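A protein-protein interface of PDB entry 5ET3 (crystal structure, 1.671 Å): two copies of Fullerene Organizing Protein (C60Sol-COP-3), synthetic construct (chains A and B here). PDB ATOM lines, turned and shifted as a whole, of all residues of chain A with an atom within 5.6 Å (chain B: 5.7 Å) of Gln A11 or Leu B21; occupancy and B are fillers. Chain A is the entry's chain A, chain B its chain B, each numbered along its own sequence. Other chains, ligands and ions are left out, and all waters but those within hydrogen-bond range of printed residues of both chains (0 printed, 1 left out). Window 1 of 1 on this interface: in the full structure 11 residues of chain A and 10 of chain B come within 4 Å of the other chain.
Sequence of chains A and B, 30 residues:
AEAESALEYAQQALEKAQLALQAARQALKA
Along chain A the printed residues that touch a printed residue of chain B span positions 7 to 11. Hydrophobic or aromatic side chains of chain B within 4 Å of the printed part of chain A: Leu B21. Among the printed residues, 8 pairs touch across the chains. Among the printed residues, no Asp or Glu carboxylate lies within 4 Å of a Lys or Arg side-chain nitrogen of the other chain.
The backbone carbonyl oxygen of Gln B18 sits at hydrogen-bond distance from the side-chain amide nitrogen of Gln A11 (3.3 Å). OE1 of Gln A11 is in hydrogen-bond range of NE2 of Gln B22 (2.5 Å).
The guanidinium group (NH1) of Arg B25 sits close to the side-chain amide nitrogen (NE2) of Gln B22 (3.2 Å).
Gln A11 touches just these residues of chain B: Gln B18 (3.3 Å), Leu B21 (3.6 Å), Gln B22 (2.5 Å) and Arg B25 (3.2 Å). Leu B21 touches just these residues of chain A: Leu A7, Ala A10 and Gln A11. Of the printed residues of chain B, Ala A10 touches Leu B21. Printed residues of chain A within 4 Å of Gln B18: Gln A11 (3.3 Å). Lys A16 touches none of the printed residues of chain B. The nearest residue of chain B that does not touch Gln A11 is Leu B19 (5.2 Å).
Position printed for both chains: 16.
Among the printed residues, merely in contact across the chains: Leu A7 with Leu B21 (3.6 Å), Leu A7 with Arg B25 (3.8 Å), Glu A8 with Arg B25 (3.8 Å), Ala A10 with Leu B21 (3.9 Å), Gln A11 with Leu B21 (3.6 Å) and Gln A11 with Arg B25 (3.2 Å).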
ATOM      1  N   ALA A   6      23.141  29.487 -18.656  1.00  0.00           N
ATOM      2  CA  ALA A   6      22.064  28.505 -18.651  1.00  0.00           C
ATOM      3  C   ALA A   6      21.726  28.081 -17.228  1.00  0.00           C
ATOM      4  O   ALA A   6      20.552  27.957 -16.876  1.00  0.00           O
ATOM      5  CB  ALA A   6      22.438  27.294 -19.484  1.00  0.00           C
ATOM      6  N   LEU A   7      22.749  27.871 -16.407  1.00  0.00           N
ATOM      7  CA  LEU A   7      22.514  27.416 -15.039  1.00  0.00           C
ATOM      8  C   LEU A   7      21.929  28.533 -14.201  1.00  0.00           C
ATOM      9  O   LEU A   7      21.092  28.286 -13.332  1.00  0.00           O
ATOM     10  CB  LEU A   7      23.804  26.897 -14.404  1.00  0.00           C
ATOM     11  CG  LEU A   7      24.387  25.638 -15.047  1.00  0.00           C
ATOM     12  CD1 LEU A   7      25.499  25.134 -14.164  1.00  0.00           C
ATOM     13  CD2 LEU A   7      23.340  24.548 -15.272  1.00  0.00           C
ATOM     14  N   GLU A   8      22.351  29.762 -14.479  1.00  0.00           N
ATOM     15  CA  GLU A   8      21.816  30.918 -13.772  1.00  0.00           C
ATOM     16  C   GLU A   8      20.324  31.079 -14.087  1.00  0.00           C
ATOM     17  O   GLU A   8      19.511  31.309 -13.196  1.00  0.00           O
ATOM     18  CB  GLU A   8      22.588  32.185 -14.148  1.00  0.00           C
ATOM     19  CG  GLU A   8      22.192  33.407 -13.330  1.00  0.00           C
ATOM     20  CD  GLU A   8      23.092  34.605 -13.583  1.00  0.00           C
ATOM     21  OE1 GLU A   8      24.156  34.436 -14.218  1.00  0.00           O
ATOM     22  OE2 GLU A   8      22.732  35.718 -13.146  1.00  0.00           O
ATOM     23  N   TYR A   9      19.974  30.932 -15.361  1.00  0.00           N
ATOM     24  CA  TYR A   9      18.589  31.017 -15.805  1.00  0.00           C
ATOM     25  C   TYR A   9      17.752  29.896 -15.193  1.00  0.00           C
ATOM     26  O   TYR A   9      16.646  30.122 -14.719  1.00  0.00           O
ATOM     27  CB  TYR A   9      18.548  30.964 -17.337  1.00  0.00           C
ATOM     28  CG  TYR A   9      17.178  30.868 -17.968  1.00  0.00           C
ATOM     29  CD1 TYR A   9      16.535  32.002 -18.448  1.00  0.00           C
ATOM     30  CD2 TYR A   9      16.545  29.642 -18.129  1.00  0.00           C
ATOM     31  CE1 TYR A   9      15.294  31.919 -19.046  1.00  0.00           C
ATOM     32  CE2 TYR A   9      15.304  29.550 -18.727  1.00  0.00           C
ATOM     33  CZ  TYR A   9      14.684  30.688 -19.187  1.00  0.00           C
ATOM     34  OH  TYR A   9      13.449  30.587 -19.786  1.00  0.00           O
ATOM     35  N   ALA A  10      18.301  28.685 -15.210  1.00  0.00           N
ATOM     36  CA  ALA A  10      17.623  27.523 -14.651  1.00  0.00           C
ATOM     37  C   ALA A  10      17.312  27.746 -13.177  1.00  0.00           C
ATOM     38  O   ALA A  10      16.210  27.459 -12.722  1.00  0.00           O
ATOM     39  CB  ALA A  10      18.481  26.278 -14.831  1.00  0.00           C
ATOM     40  N   GLN A  11      18.289  28.273 -12.443  1.00  0.00           N
ATOM     41  CA  GLN A  11      18.115  28.539 -11.016  1.00  0.00           C
ATOM     42  C   GLN A  11      17.025  29.585 -10.785  1.00  0.00           C
ATOM     43  O   GLN A  11      16.205  29.453  -9.876  1.00  0.00           O
ATOM     44  CB  GLN A  11      19.427  29.008 -10.398  1.00  0.00           C
ATOM     45  CG  GLN A  11      19.460  28.947  -8.887  1.00  0.00           C
ATOM     46  CD  GLN A  11      20.336  27.815  -8.383  1.00  0.00           C
ATOM     47  OE1 GLN A  11      21.521  27.744  -8.705  1.00  0.00           O
ATOM     48  NE2 GLN A  11      19.755  26.918  -7.595  1.00  0.00           N
ATOM     49  N   GLN A  12      17.010  30.613 -11.623  1.00  0.00           N
ATOM     50  CA  GLN A  12      15.991  31.653 -11.530  1.00  0.00           C
ATOM     51  C   GLN A  12      14.598  31.103 -11.858  1.00  0.00           C
ATOM     52  O   GLN A  12      13.628  31.421 -11.183  1.00  0.00           O
ATOM     53  CB  GLN A  12      16.344  32.818 -12.456  1.00  0.00           C
ATOM     54  CG  GLN A  12      17.558  33.604 -11.980  1.00  0.00           C
ATOM     55  CD  GLN A  12      18.169  34.491 -13.049  1.00  0.00           C
ATOM     56  OE1 GLN A  12      17.794  34.433 -14.219  1.00  0.00           O
ATOM     57  NE2 GLN A  12      19.127  35.318 -12.645  1.00  0.00           N
ATOM     58  N   ALA A  13      14.511  30.262 -12.884  1.00  0.00           N
ATOM     59  CA  ALA A  13      13.267  29.590 -13.236  1.00  0.00           C
ATOM     60  C   ALA A  13      12.742  28.714 -12.097  1.00  0.00           C
ATOM     61  O   ALA A  13      11.544  28.711 -11.820  1.00  0.00           O
ATOM     62  CB  ALA A  13      13.457  28.750 -14.500  1.00  0.00           C
ATOM     63  N   LEU A  14      13.634  27.986 -11.437  1.00  0.00           N
ATOM     64  CA  LEU A  14      13.235  27.125 -10.330  1.00  0.00           C
ATOM     65  C   LEU A  14      12.754  27.954  -9.135  1.00  0.00           C
ATOM     66  O   LEU A  14      11.805  27.560  -8.466  1.00  0.00           O
ATOM     67  CB  LEU A  14      14.388  26.205  -9.913  1.00  0.00           C
ATOM     68  CG  LEU A  14      14.800  25.114 -10.909  1.00  0.00           C
ATOM     69  CD1 LEU A  14      15.788  24.170 -10.237  1.00  0.00           C
ATOM     70  CD2 LEU A  14      13.609  24.349 -11.469  1.00  0.00           C
ATOM     71  N   GLU A  15      13.400  29.091  -8.883  1.00  0.00           N
ATOM     72  CA  GLU A  15      12.974  30.020  -7.835  1.00  0.00           C
ATOM     73  C   GLU A  15      11.533  30.468  -8.073  1.00  0.00           C
ATOM     74  O   GLU A  15      10.716  30.513  -7.141  1.00  0.00           O
ATOM     75  CB  GLU A  15      13.904  31.238  -7.773  1.00  0.00           C
ATOM     76  CG  GLU A  15      15.196  30.983  -7.024  1.00  0.00           C
ATOM     77  CD  GLU A  15      16.237  32.061  -7.246  1.00  0.00           C
ATOM     78  OE1 GLU A  15      15.912  33.093  -7.873  1.00  0.00           O
ATOM     79  OE2 GLU A  15      17.386  31.870  -6.793  1.00  0.00           O
ATOM     80  N   LYS A  16      11.226  30.762  -9.333  1.00  0.00           N
ATOM     81  CA  LYS A  16       9.887  31.182  -9.724  1.00  0.00           C
ATOM     82  C   LYS A  16       8.887  30.050  -9.507  1.00  0.00           C
ATOM     83  O   LYS A  16       7.781  30.279  -9.018  1.00  0.00           O
ATOM     84  CB  LYS A  16       9.869  31.620 -11.190  1.00  0.00           C
ATOM     85  CG  LYS A  16      10.484  32.989 -11.434  1.00  0.00           C
ATOM     86  CD  LYS A  16      10.570  33.303 -12.919  1.00  0.00           C
ATOM     87  CE  LYS A  16      11.378  34.564 -13.174  1.00  0.00           C
ATOM     88  NZ  LYS A  16      11.451  34.899 -14.623  1.00  0.00           N
ATOM     89  N   LYS B  16      15.894  19.758  -3.886  1.00  0.00           N
ATOM     90  CA  LYS B  16      17.023  18.903  -4.234  1.00  0.00           C
ATOM     91  C   LYS B  16      17.663  19.314  -5.563  1.00  0.00           C
ATOM     92  O   LYS B  16      18.882  19.295  -5.703  1.00  0.00           O
ATOM     93  CB  LYS B  16      16.579  17.445  -4.280  1.00  0.00           C
ATOM     94  CG  LYS B  16      16.163  16.915  -2.922  1.00  0.00           C
ATOM     95  CD  LYS B  16      15.647  15.492  -2.995  1.00  0.00           C
ATOM     96  CE  LYS B  16      15.140  15.048  -1.630  1.00  0.00           C
ATOM     97  NZ  LYS B  16      14.585  13.668  -1.652  1.00  0.00           N
ATOM     98  N   ALA B  17      16.848  19.701  -6.538  1.00  0.00           N
ATOM     99  CA  ALA B  17      17.388  20.182  -7.802  1.00  0.00           C
ATOM    100  C   ALA B  17      18.213  21.441  -7.577  1.00  0.00           C
ATOM    101  O   ALA B  17      19.251  21.637  -8.207  1.00  0.00           O
ATOM    102  CB  ALA B  17      16.271  20.460  -8.793  1.00  0.00           C
ATOM    103  N   GLN B  18      17.752  22.289  -6.666  1.00  0.00           N
ATOM    104  CA  GLN B  18      18.397  23.573  -6.447  1.00  0.00           C
ATOM    105  C   GLN B  18      19.760  23.412  -5.813  1.00  0.00           C
ATOM    106  O   GLN B  18      20.706  24.117  -6.182  1.00  0.00           O
ATOM    107  CB  GLN B  18      17.537  24.459  -5.573  1.00  0.00           C
ATOM    108  CG  GLN B  18      16.342  24.993  -6.276  1.00  0.00           C
ATOM    109  CD  GLN B  18      15.466  25.733  -5.332  1.00  0.00           C
ATOM    110  OE1 GLN B  18      14.812  25.132  -4.480  1.00  0.00           O
ATOM    111  NE2 GLN B  18      15.456  27.054  -5.446  1.00  0.00           N
ATOM    112  N   LEU B  19      19.875  22.497  -4.857  1.00  0.00           N
ATOM    113  CA  LEU B  19      21.153  22.330  -4.173  1.00  0.00           C
ATOM    114  C   LEU B  19      22.174  21.665  -5.099  1.00  0.00           C
ATOM    115  O   LEU B  19      23.357  21.988  -5.040  1.00  0.00           O
ATOM    116  CB  LEU B  19      20.980  21.550  -2.862  1.00  0.00           C
ATOM    117  CG  LEU B  19      20.497  20.098  -2.840  1.00  0.00           C
ATOM    118  CD1 LEU B  19      21.669  19.146  -2.986  1.00  0.00           C
ATOM    119  CD2 LEU B  19      19.732  19.797  -1.556  1.00  0.00           C
ATOM    120  N   ALA B  20      21.718  20.762  -5.967  1.00  0.00           N
ATOM    121  CA  ALA B  20      22.597  20.157  -6.964  1.00  0.00           C
ATOM    122  C   ALA B  20      23.018  21.198  -8.002  1.00  0.00           C
ATOM    123  O   ALA B  20      24.161  21.201  -8.461  1.00  0.00           O
ATOM    124  CB  ALA B  20      21.912  18.978  -7.643  1.00  0.00           C
ATOM    125  N   LEU B  21      22.103  22.099  -8.337  1.00  0.00           N
ATOM    126  CA  LEU B  21      22.398  23.156  -9.293  1.00  0.00           C
ATOM    127  C   LEU B  21      23.475  24.082  -8.732  1.00  0.00           C
ATOM    128  O   LEU B  21      24.358  24.532  -9.463  1.00  0.00           O
ATOM    129  CB  LEU B  21      21.135  23.955  -9.615  1.00  0.00           C
ATOM    130  CG  LEU B  21      21.232  24.884 -10.827  1.00  0.00           C
ATOM    131  CD1 LEU B  21      22.016  24.218 -11.949  1.00  0.00           C
ATOM    132  CD2 LEU B  21      19.847  25.290 -11.303  1.00  0.00           C
ATOM    133  N   GLN B  22      23.399  24.366  -7.433  1.00  0.00           N
ATOM    134  CA  GLN B  22      24.373  25.247  -6.785  1.00  0.00           C
ATOM    135  C   GLN B  22      25.758  24.614  -6.764  1.00  0.00           C
ATOM    136  O   GLN B  22      26.765  25.303  -6.941  1.00  0.00           O
ATOM    137  CB  GLN B  22      23.932  25.593  -5.361  1.00  0.00           C
ATOM    138  CG  GLN B  22      22.911  26.725  -5.292  1.00  0.00           C
ATOM    139  CD  GLN B  22      23.508  28.053  -5.726  1.00  0.00           C
ATOM    140  OE1 GLN B  22      24.293  28.661  -4.998  1.00  0.00           O
ATOM    141  NE2 GLN B  22      23.156  28.494  -6.923  1.00  0.00           N
ATOM    142  N   ALA B  23      25.808  23.306  -6.534  1.00  0.00           N
ATOM    143  CA  ALA B  23      27.065  22.571  -6.604  1.00  0.00           C
ATOM    144  C   ALA B  23      27.658  22.669  -8.010  1.00  0.00           C
ATOM    145  O   ALA B  23      28.853  22.891  -8.175  1.00  0.00           O
ATOM    146  CB  ALA B  23      26.853  21.118  -6.220  1.00  0.00           C
ATOM    147  N   ALA B  24      26.808  22.507  -9.022  1.00  0.00           N
ATOM    148  CA  ALA B  24      27.255  22.564 -10.411  1.00  0.00           C
ATOM    149  C   ALA B  24      27.761  23.953 -10.779  1.00  0.00           C
ATOM    150  O   ALA B  24      28.765  24.091 -11.479  1.00  0.00           O
ATOM    151  CB  ALA B  24      26.134  22.150 -11.350  1.00  0.00           C
ATOM    152  N   ARG B  25      27.067  24.988 -10.314  1.00  0.00           N
ATOM    153  CA  ARG B  25      27.495  26.351 -10.611  1.00  0.00           C
ATOM    154  C   ARG B  25      28.858  26.634  -9.983  1.00  0.00           C
ATOM    155  O   ARG B  25      29.713  27.264 -10.610  1.00  0.00           O
ATOM    156  CB  ARG B  25      26.459  27.356 -10.129  1.00  0.00           C
ATOM    157  CG  ARG B  25      25.169  27.268 -10.923  1.00  0.00           C
ATOM    158  CD  ARG B  25      24.176  28.314 -10.489  1.00  0.00           C
ATOM    159  NE  ARG B  25      24.582  29.655 -10.895  1.00  0.00           N
ATOM    160  CZ  ARG B  25      24.162  30.773 -10.312  1.00  0.00           C
ATOM    161  NH1 ARG B  25      23.330  30.717  -9.279  1.00  0.00           N
ATOM    162  NH2 ARG B  25      24.583  31.948 -10.754  1.00  0.00           N
ATOM    163  N   GLN B  26      29.065  26.156  -8.760  1.00  0.00           N
ATOM    164  CA  GLN B  26      30.368  26.288  -8.104  1.00  0.00           C
ATOM    165  C   GLN B  26      31.456  25.542  -8.881  1.00  0.00           C
ATOM    166  O   GLN B  26      32.565  26.054  -9.064  1.00  0.00           O
ATOM    167  CB  GLN B  26      30.293  25.774  -6.663  1.00  0.00           C
ATOM    168  CG  GLN B  26      31.605  25.848  -5.891  1.00  0.00           C
ATOM    169  CD  GLN B  26      32.130  27.265  -5.775  1.00  0.00           C
ATOM    170  OE1 GLN B  26      31.357  28.218  -5.682  1.00  0.00           O
ATOM    171  NE2 GLN B  26      33.450  27.410  -5.784  1.00  0.00           N
